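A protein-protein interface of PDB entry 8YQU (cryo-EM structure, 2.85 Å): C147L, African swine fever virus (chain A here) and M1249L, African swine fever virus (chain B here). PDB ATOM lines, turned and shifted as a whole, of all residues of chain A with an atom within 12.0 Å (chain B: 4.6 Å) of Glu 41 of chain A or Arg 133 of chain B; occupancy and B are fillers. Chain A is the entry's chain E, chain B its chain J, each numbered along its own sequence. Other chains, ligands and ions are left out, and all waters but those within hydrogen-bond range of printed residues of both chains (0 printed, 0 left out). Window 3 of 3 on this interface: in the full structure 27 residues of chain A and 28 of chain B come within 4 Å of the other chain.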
ATOM      1  N   ILE A  39      -7.852  33.707   7.855  1.00  0.00           N
ATOM      2  CA  ILE A  39      -6.647  33.436   8.629  1.00  0.00           C
ATOM      3  C   ILE A  39      -6.141  32.028   8.343  1.00  0.00           C
ATOM      4  O   ILE A  39      -6.830  31.045   8.619  1.00  0.00           O
ATOM      5  CB  ILE A  39      -6.897  33.628  10.135  1.00  0.00           C
ATOM      6  CG1 ILE A  39      -7.261  35.082  10.438  1.00  0.00           C
ATOM      7  CG2 ILE A  39      -5.677  33.203  10.937  1.00  0.00           C
ATOM      8  CD1 ILE A  39      -7.773  35.302  11.843  1.00  0.00           C
ATOM      9  N   VAL A  40      -4.934  31.933   7.792  1.00  0.00           N
ATOM     10  CA  VAL A  40      -4.315  30.640   7.521  1.00  0.00           C
ATOM     11  C   VAL A  40      -3.758  30.113   8.839  1.00  0.00           C
ATOM     12  O   VAL A  40      -2.825  30.687   9.406  1.00  0.00           O
ATOM     13  CB  VAL A  40      -3.220  30.748   6.455  1.00  0.00           C
ATOM     14  CG1 VAL A  40      -2.546  29.403   6.266  1.00  0.00           C
ATOM     15  CG2 VAL A  40      -3.806  31.245   5.143  1.00  0.00           C
ATOM     16  N   GLU A  41      -4.329  29.020   9.325  1.00  0.00           N
ATOM     17  CA  GLU A  41      -4.138  28.567  10.691  1.00  0.00           C
ATOM     18  C   GLU A  41      -3.068  27.480  10.776  1.00  0.00           C
ATOM     19  O   GLU A  41      -2.338  27.208   9.819  1.00  0.00           O
ATOM     20  CB  GLU A  41      -5.479  28.094  11.247  1.00  0.00           C
ATOM     21  CG  GLU A  41      -6.468  29.224  11.419  1.00  0.00           C
ATOM     22  CD  GLU A  41      -7.802  28.753  11.935  1.00  0.00           C
ATOM     23  OE1 GLU A  41      -7.997  27.523  12.036  1.00  0.00           O
ATOM     24  OE2 GLU A  41      -8.655  29.614  12.233  1.00  0.00           O
ATOM     25  N   SER A  42      -2.977  26.854  11.948  1.00  0.00           N
ATOM     26  CA  SER A  42      -1.949  25.864  12.213  1.00  0.00           C
ATOM     27  C   SER A  42      -2.155  24.624  11.340  1.00  0.00           C
ATOM     28  O   SER A  42      -3.278  24.334  10.916  1.00  0.00           O
ATOM     29  CB  SER A  42      -1.970  25.472  13.687  1.00  0.00           C
ATOM     30  OG  SER A  42      -1.651  26.581  14.511  1.00  0.00           O
ATOM     31  N   PRO A  43      -1.084  23.884  11.049  1.00  0.00           N
ATOM     32  CA  PRO A  43      -1.221  22.690  10.207  1.00  0.00           C
ATOM     33  C   PRO A  43      -2.139  21.654  10.839  1.00  0.00           C
ATOM     34  O   PRO A  43      -2.168  21.481  12.060  1.00  0.00           O
ATOM     35  CB  PRO A  43       0.216  22.170  10.087  1.00  0.00           C
ATOM     36  CG  PRO A  43       0.958  22.800  11.220  1.00  0.00           C
ATOM     37  CD  PRO A  43       0.315  24.130  11.437  1.00  0.00           C
ATOM     38  N   SER A  44      -2.890  20.962   9.990  1.00  0.00           N
ATOM     39  CA  SER A  44      -3.834  19.939  10.404  1.00  0.00           C
ATOM     40  C   SER A  44      -3.362  18.571   9.918  1.00  0.00           C
ATOM     41  O   SER A  44      -2.277  18.428   9.341  1.00  0.00           O
ATOM     42  CB  SER A  44      -5.233  20.275   9.883  1.00  0.00           C
ATOM     43  OG  SER A  44      -5.238  20.385   8.470  1.00  0.00           O
ATOM     44  N   ILE A  45      -4.189  17.553  10.154  1.00  0.00           N
ATOM     45  CA  ILE A  45      -3.855  16.195   9.744  1.00  0.00           C
ATOM     46  C   ILE A  45      -4.243  15.920   8.294  1.00  0.00           C
ATOM     47  O   ILE A  45      -3.670  15.015   7.669  1.00  0.00           O
ATOM     48  CB  ILE A  45      -4.521  15.188  10.700  1.00  0.00           C
ATOM     49  CG1 ILE A  45      -4.174  15.543  12.146  1.00  0.00           C
ATOM     50  CG2 ILE A  45      -4.065  13.765  10.413  1.00  0.00           C
ATOM     51  CD1 ILE A  45      -5.048  14.866  13.172  1.00  0.00           C
ATOM     52  N   CYS A  46      -5.178  16.691   7.733  1.00  0.00           N
ATOM     53  CA  CYS A  46      -5.538  16.518   6.328  1.00  0.00           C
ATOM     54  C   CYS A  46      -4.344  16.777   5.420  1.00  0.00           C
ATOM     55  O   CYS A  46      -4.145  16.072   4.424  1.00  0.00           O
ATOM     56  CB  CYS A  46      -6.702  17.439   5.966  1.00  0.00           C
ATOM     57  SG  CYS A  46      -6.323  19.203   6.073  1.00  0.00           S
ATOM     58  N   GLU A  47      -3.549  17.792   5.736  1.00  0.00           N
ATOM     59  CA  GLU A  47      -2.297  18.036   5.042  1.00  0.00           C
ATOM     60  C   GLU A  47      -1.138  17.397   5.806  1.00  0.00           C
ATOM     61  O   GLU A  47      -1.244  17.062   6.987  1.00  0.00           O
ATOM     62  CB  GLU A  47      -2.070  19.537   4.866  1.00  0.00           C
ATOM     63  CG  GLU A  47      -1.886  20.290   6.172  1.00  0.00           C
ATOM     64  CD  GLU A  47      -1.736  21.784   5.964  1.00  0.00           C
ATOM     65  OE1 GLU A  47      -1.795  22.235   4.801  1.00  0.00           O
ATOM     66  OE2 GLU A  47      -1.565  22.508   6.966  1.00  0.00           O
ATOM     67  N   GLY A  48      -0.017  17.229   5.112  1.00  0.00           N
ATOM     68  CA  GLY A  48       1.162  16.640   5.710  1.00  0.00           C
ATOM     69  C   GLY A  48       1.329  15.153   5.494  1.00  0.00           C
ATOM     70  O   GLY A  48       2.196  14.548   6.134  1.00  0.00           O
ATOM     71  N   ASP B  87      -4.312  22.307  18.553  1.00  0.00           N
ATOM     72  CA  ASP B  87      -4.361  23.516  17.736  1.00  0.00           C
ATOM     73  C   ASP B  87      -5.749  24.140  17.720  1.00  0.00           C
ATOM     74  O   ASP B  87      -5.875  25.340  17.454  1.00  0.00           O
ATOM     75  CB  ASP B  87      -3.911  23.207  16.307  1.00  0.00           C
ATOM     76  CG  ASP B  87      -2.414  23.006  16.198  1.00  0.00           C
ATOM     77  OD1 ASP B  87      -1.689  23.411  17.131  1.00  0.00           O
ATOM     78  OD2 ASP B  87      -1.961  22.445  15.177  1.00  0.00           O
ATOM     79  N   VAL B  88      -6.787  23.352  17.992  1.00  0.00           N
ATOM     80  CA  VAL B  88      -8.144  23.856  18.167  1.00  0.00           C
ATOM     81  C   VAL B  88      -8.221  24.580  19.504  1.00  0.00           C
ATOM     82  O   VAL B  88      -7.252  24.585  20.272  1.00  0.00           O
ATOM     83  CB  VAL B  88      -9.186  22.726  18.079  1.00  0.00           C
ATOM     84  CG1 VAL B  88      -8.963  21.896  16.825  1.00  0.00           C
ATOM     85  CG2 VAL B  88      -9.134  21.854  19.321  1.00  0.00           C
ATOM     86  N   PRO B  90      -8.333  28.039  20.598  1.00  0.00           N
ATOM     87  CA  PRO B  90      -7.406  29.081  21.048  1.00  0.00           C
ATOM     88  C   PRO B  90      -8.048  29.991  22.080  1.00  0.00           C
ATOM     89  O   PRO B  90      -9.160  29.726  22.548  1.00  0.00           O
ATOM     90  CB  PRO B  90      -7.062  29.828  19.751  1.00  0.00           C
ATOM     91  CG  PRO B  90      -8.095  29.360  18.721  1.00  0.00           C
ATOM     92  CD  PRO B  90      -9.096  28.504  19.433  1.00  0.00           C
ATOM     93  N   PHE B 110      -6.320  34.846  19.927  1.00  0.00           N
ATOM     94  CA  PHE B 110      -7.048  36.032  19.509  1.00  0.00           C
ATOM     95  C   PHE B 110      -7.174  36.987  20.692  1.00  0.00           C
ATOM     96  O   PHE B 110      -6.806  36.668  21.825  1.00  0.00           O
ATOM     97  CB  PHE B 110      -8.425  35.654  18.961  1.00  0.00           C
ATOM     98  CG  PHE B 110      -8.381  34.896  17.666  1.00  0.00           C
ATOM     99  CD1 PHE B 110      -7.581  35.326  16.621  1.00  0.00           C
ATOM    100  CD2 PHE B 110      -9.133  33.746  17.495  1.00  0.00           C
ATOM    101  CE1 PHE B 110      -7.545  34.630  15.429  1.00  0.00           C
ATOM    102  CE2 PHE B 110      -9.096  33.045  16.308  1.00  0.00           C
ATOM    103  CZ  PHE B 110      -8.300  33.486  15.273  1.00  0.00           C
ATOM    104  N   LYS B 131     -13.087  29.485  21.976  1.00  0.00           N
ATOM    105  CA  LYS B 131     -13.728  29.203  20.691  1.00  0.00           C
ATOM    106  C   LYS B 131     -13.177  27.878  20.172  1.00  0.00           C
ATOM    107  O   LYS B 131     -11.985  27.777  19.881  1.00  0.00           O
ATOM    108  CB  LYS B 131     -13.482  30.321  19.686  1.00  0.00           C
ATOM    109  CG  LYS B 131     -14.196  30.094  18.360  1.00  0.00           C
ATOM    110  CD  LYS B 131     -13.998  31.247  17.394  1.00  0.00           C
ATOM    111  CE  LYS B 131     -14.711  30.984  16.077  1.00  0.00           C
ATOM    112  NZ  LYS B 131     -14.524  32.096  15.106  1.00  0.00           N
ATOM    113  N   LEU B 132     -14.046  26.883  20.041  1.00  0.00           N
ATOM    114  CA  LEU B 132     -13.669  25.673  19.322  1.00  0.00           C
ATOM    115  C   LEU B 132     -14.024  25.823  17.851  1.00  0.00           C
ATOM    116  O   LEU B 132     -15.177  26.097  17.509  1.00  0.00           O
ATOM    117  CB  LEU B 132     -14.352  24.437  19.904  1.00  0.00           C
ATOM    118  CG  LEU B 132     -13.905  23.117  19.267  1.00  0.00           C
ATOM    119  CD1 LEU B 132     -13.701  22.049  20.313  1.00  0.00           C
ATOM    120  CD2 LEU B 132     -14.923  22.640  18.238  1.00  0.00           C
ATOM    121  N   ARG B 133     -13.035  25.630  16.987  1.00  0.00           N
ATOM    122  CA  ARG B 133     -13.236  25.745  15.553  1.00  0.00           C
ATOM    123  C   ARG B 133     -13.793  24.447  14.992  1.00  0.00           C
ATOM    124  O   ARG B 133     -13.347  23.355  15.354  1.00  0.00           O
ATOM    125  CB  ARG B 133     -11.925  26.089  14.850  1.00  0.00           C
ATOM    126  CG  ARG B 133     -11.475  27.517  15.045  1.00  0.00           C
ATOM    127  CD  ARG B 133     -10.359  27.830  14.083  1.00  0.00           C
ATOM    128  NE  ARG B 133      -9.137  27.105  14.411  1.00  0.00           N
ATOM    129  CZ  ARG B 133      -8.132  27.610  15.112  1.00  0.00           C
ATOM    130  NH1 ARG B 133      -8.152  28.858  15.549  1.00  0.00           N
ATOM    131  NH2 ARG B 133      -7.075  26.846  15.373  1.00  0.00           N
ATOM    132  N   LEU B 134     -14.777  24.576  14.105  1.00  0.00           N
ATOM    133  CA  LEU B 134     -15.344  23.429  13.401  1.00  0.00           C
ATOM    134  C   LEU B 134     -14.633  23.318  12.056  1.00  0.00           C
ATOM    135  O   LEU B 134     -15.125  23.758  11.017  1.00  0.00           O
ATOM    136  CB  LEU B 134     -16.856  23.575  13.244  1.00  0.00           C
ATOM    137  CG  LEU B 134     -17.731  23.084  14.403  1.00  0.00           C
ATOM    138  CD1 LEU B 134     -17.559  21.586  14.595  1.00  0.00           C
ATOM    139  CD2 LEU B 134     -17.448  23.833  15.699  1.00  0.00           C
ATOM    140  N   LYS B 135     -13.442  22.723  12.093  1.00  0.00           N
ATOM    141  CA  LYS B 135     -12.647  22.564  10.884  1.00  0.00           C
ATOM    142  C   LYS B 135     -13.355  21.629   9.913  1.00  0.00           C
ATOM    143  O   LYS B 135     -13.753  20.521  10.281  1.00  0.00           O
ATOM    144  CB  LYS B 135     -11.262  22.017  11.227  1.00  0.00           C
ATOM    145  CG  LYS B 135     -10.519  22.814  12.284  1.00  0.00           C
ATOM    146  CD  LYS B 135      -9.015  22.673  12.114  1.00  0.00           C
ATOM    147  CE  LYS B 135      -8.278  23.035  13.391  1.00  0.00           C
ATOM    148  NZ  LYS B 135      -7.968  24.488  13.464  1.00  0.00           N
ATOM    149  N   GLU B 186     -15.912  29.002  11.237  1.00  0.00           N
ATOM    150  CA  GLU B 186     -17.035  28.539  12.036  1.00  0.00           C
ATOM    151  C   GLU B 186     -16.539  27.953  13.352  1.00  0.00           C
ATOM    152  O   GLU B 186     -15.430  27.420  13.439  1.00  0.00           O
ATOM    153  CB  GLU B 186     -17.837  27.486  11.271  1.00  0.00           C
ATOM    154  CG  GLU B 186     -18.465  27.985   9.981  1.00  0.00           C
ATOM    155  CD  GLU B 186     -19.181  26.884   9.221  1.00  0.00           C
ATOM    156  OE1 GLU B 186     -19.050  25.706   9.614  1.00  0.00           O
ATOM    157  OE2 GLU B 186     -19.874  27.198   8.230  1.00  0.00           O
ATOM    158  N   GLY B 187     -17.366  28.061  14.382  1.00  0.00           N
ATOM    159  CA  GLY B 187     -17.001  27.483  15.661  1.00  0.00           C
ATOM    160  C   GLY B 187     -18.004  27.835  16.735  1.00  0.00           C
ATOM    161  O   GLY B 187     -18.912  28.652  16.539  1.00  0.00           O
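The side-chain carboxylate (OE1) of Glu 41 of chain A is in salt-bridge range of the guanidinium group (NE) of Arg 133 of chain B (2.7 Å).
The side-chain carboxylate of Glu 41 of chain A is in salt-bridge range of the side-chain amino group of Lys 135 of chain B (3.4 Å).
The backbone carbonyl oxygen (O) of Pro 43 of chain A sits close to the side-chain carboxylate (OD2) of Asp 87 of chain B.
O of Asp 87 of chain B sits at hydrogen-bond distance from NH2 of Arg 133 of chain B (2.8 Å).
Among the printed residues, pairs that only touch across the chains: Ser 42 of chain A with Asp 87 of chain B and Ile 39 of chain A with Phe 110 of chain B.
Glu 41 of chain A touches just these residues of chain B: Arg 133 (2.7 Å) and Lys 135 (3.4 Å).
Arg 133 of chain B touches just one residue of chain A: Glu 41 (2.7 Å).
Val 88 of chain B touches none of the printed residues of chain A.
No residue of chain A comes within 4 Å of Pro 90 of chain B.
No residue of chain A comes within 4 Å of Lys 131 of chain B.
No residue of chain A comes within 4 Å of Leu 132 of chain B.
No residue of chain A comes within 4 Å of Leu 134 of chain B.
No residue of chain A comes within 4 Å of Gly 187 of chain B.
Printed residues of chain A within 4 Å of Phe 110 of chain B: Ile 39.
Of the printed residues of chain B, Ser 42 of chain A touches Asp 87.
Ile 45 of chain A touches none of the printed residues of chain B.
The nearest printed residue of chain B that does not touch Glu 41 of chain A is Phe 110 of chain B (4.9 Å).
The nearest residue of chain A that does not touch Arg 133 of chain B is Ser 42 of chain A (5.3 Å).
Of the 10 printed residues of chain A, 4 touch a printed residue of chain B.
Hydrophobic or aromatic side chains of chain A within 4 Å of the printed part of chain B: Ile 39.
Of the 11 printed residues of chain B, 4 touch a printed residue of chain A.
Hydrophobic or aromatic side chains of chain B that line the printed part of chain A: Phe 110.
Among the printed residues, 5 pairs touch across the chains.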
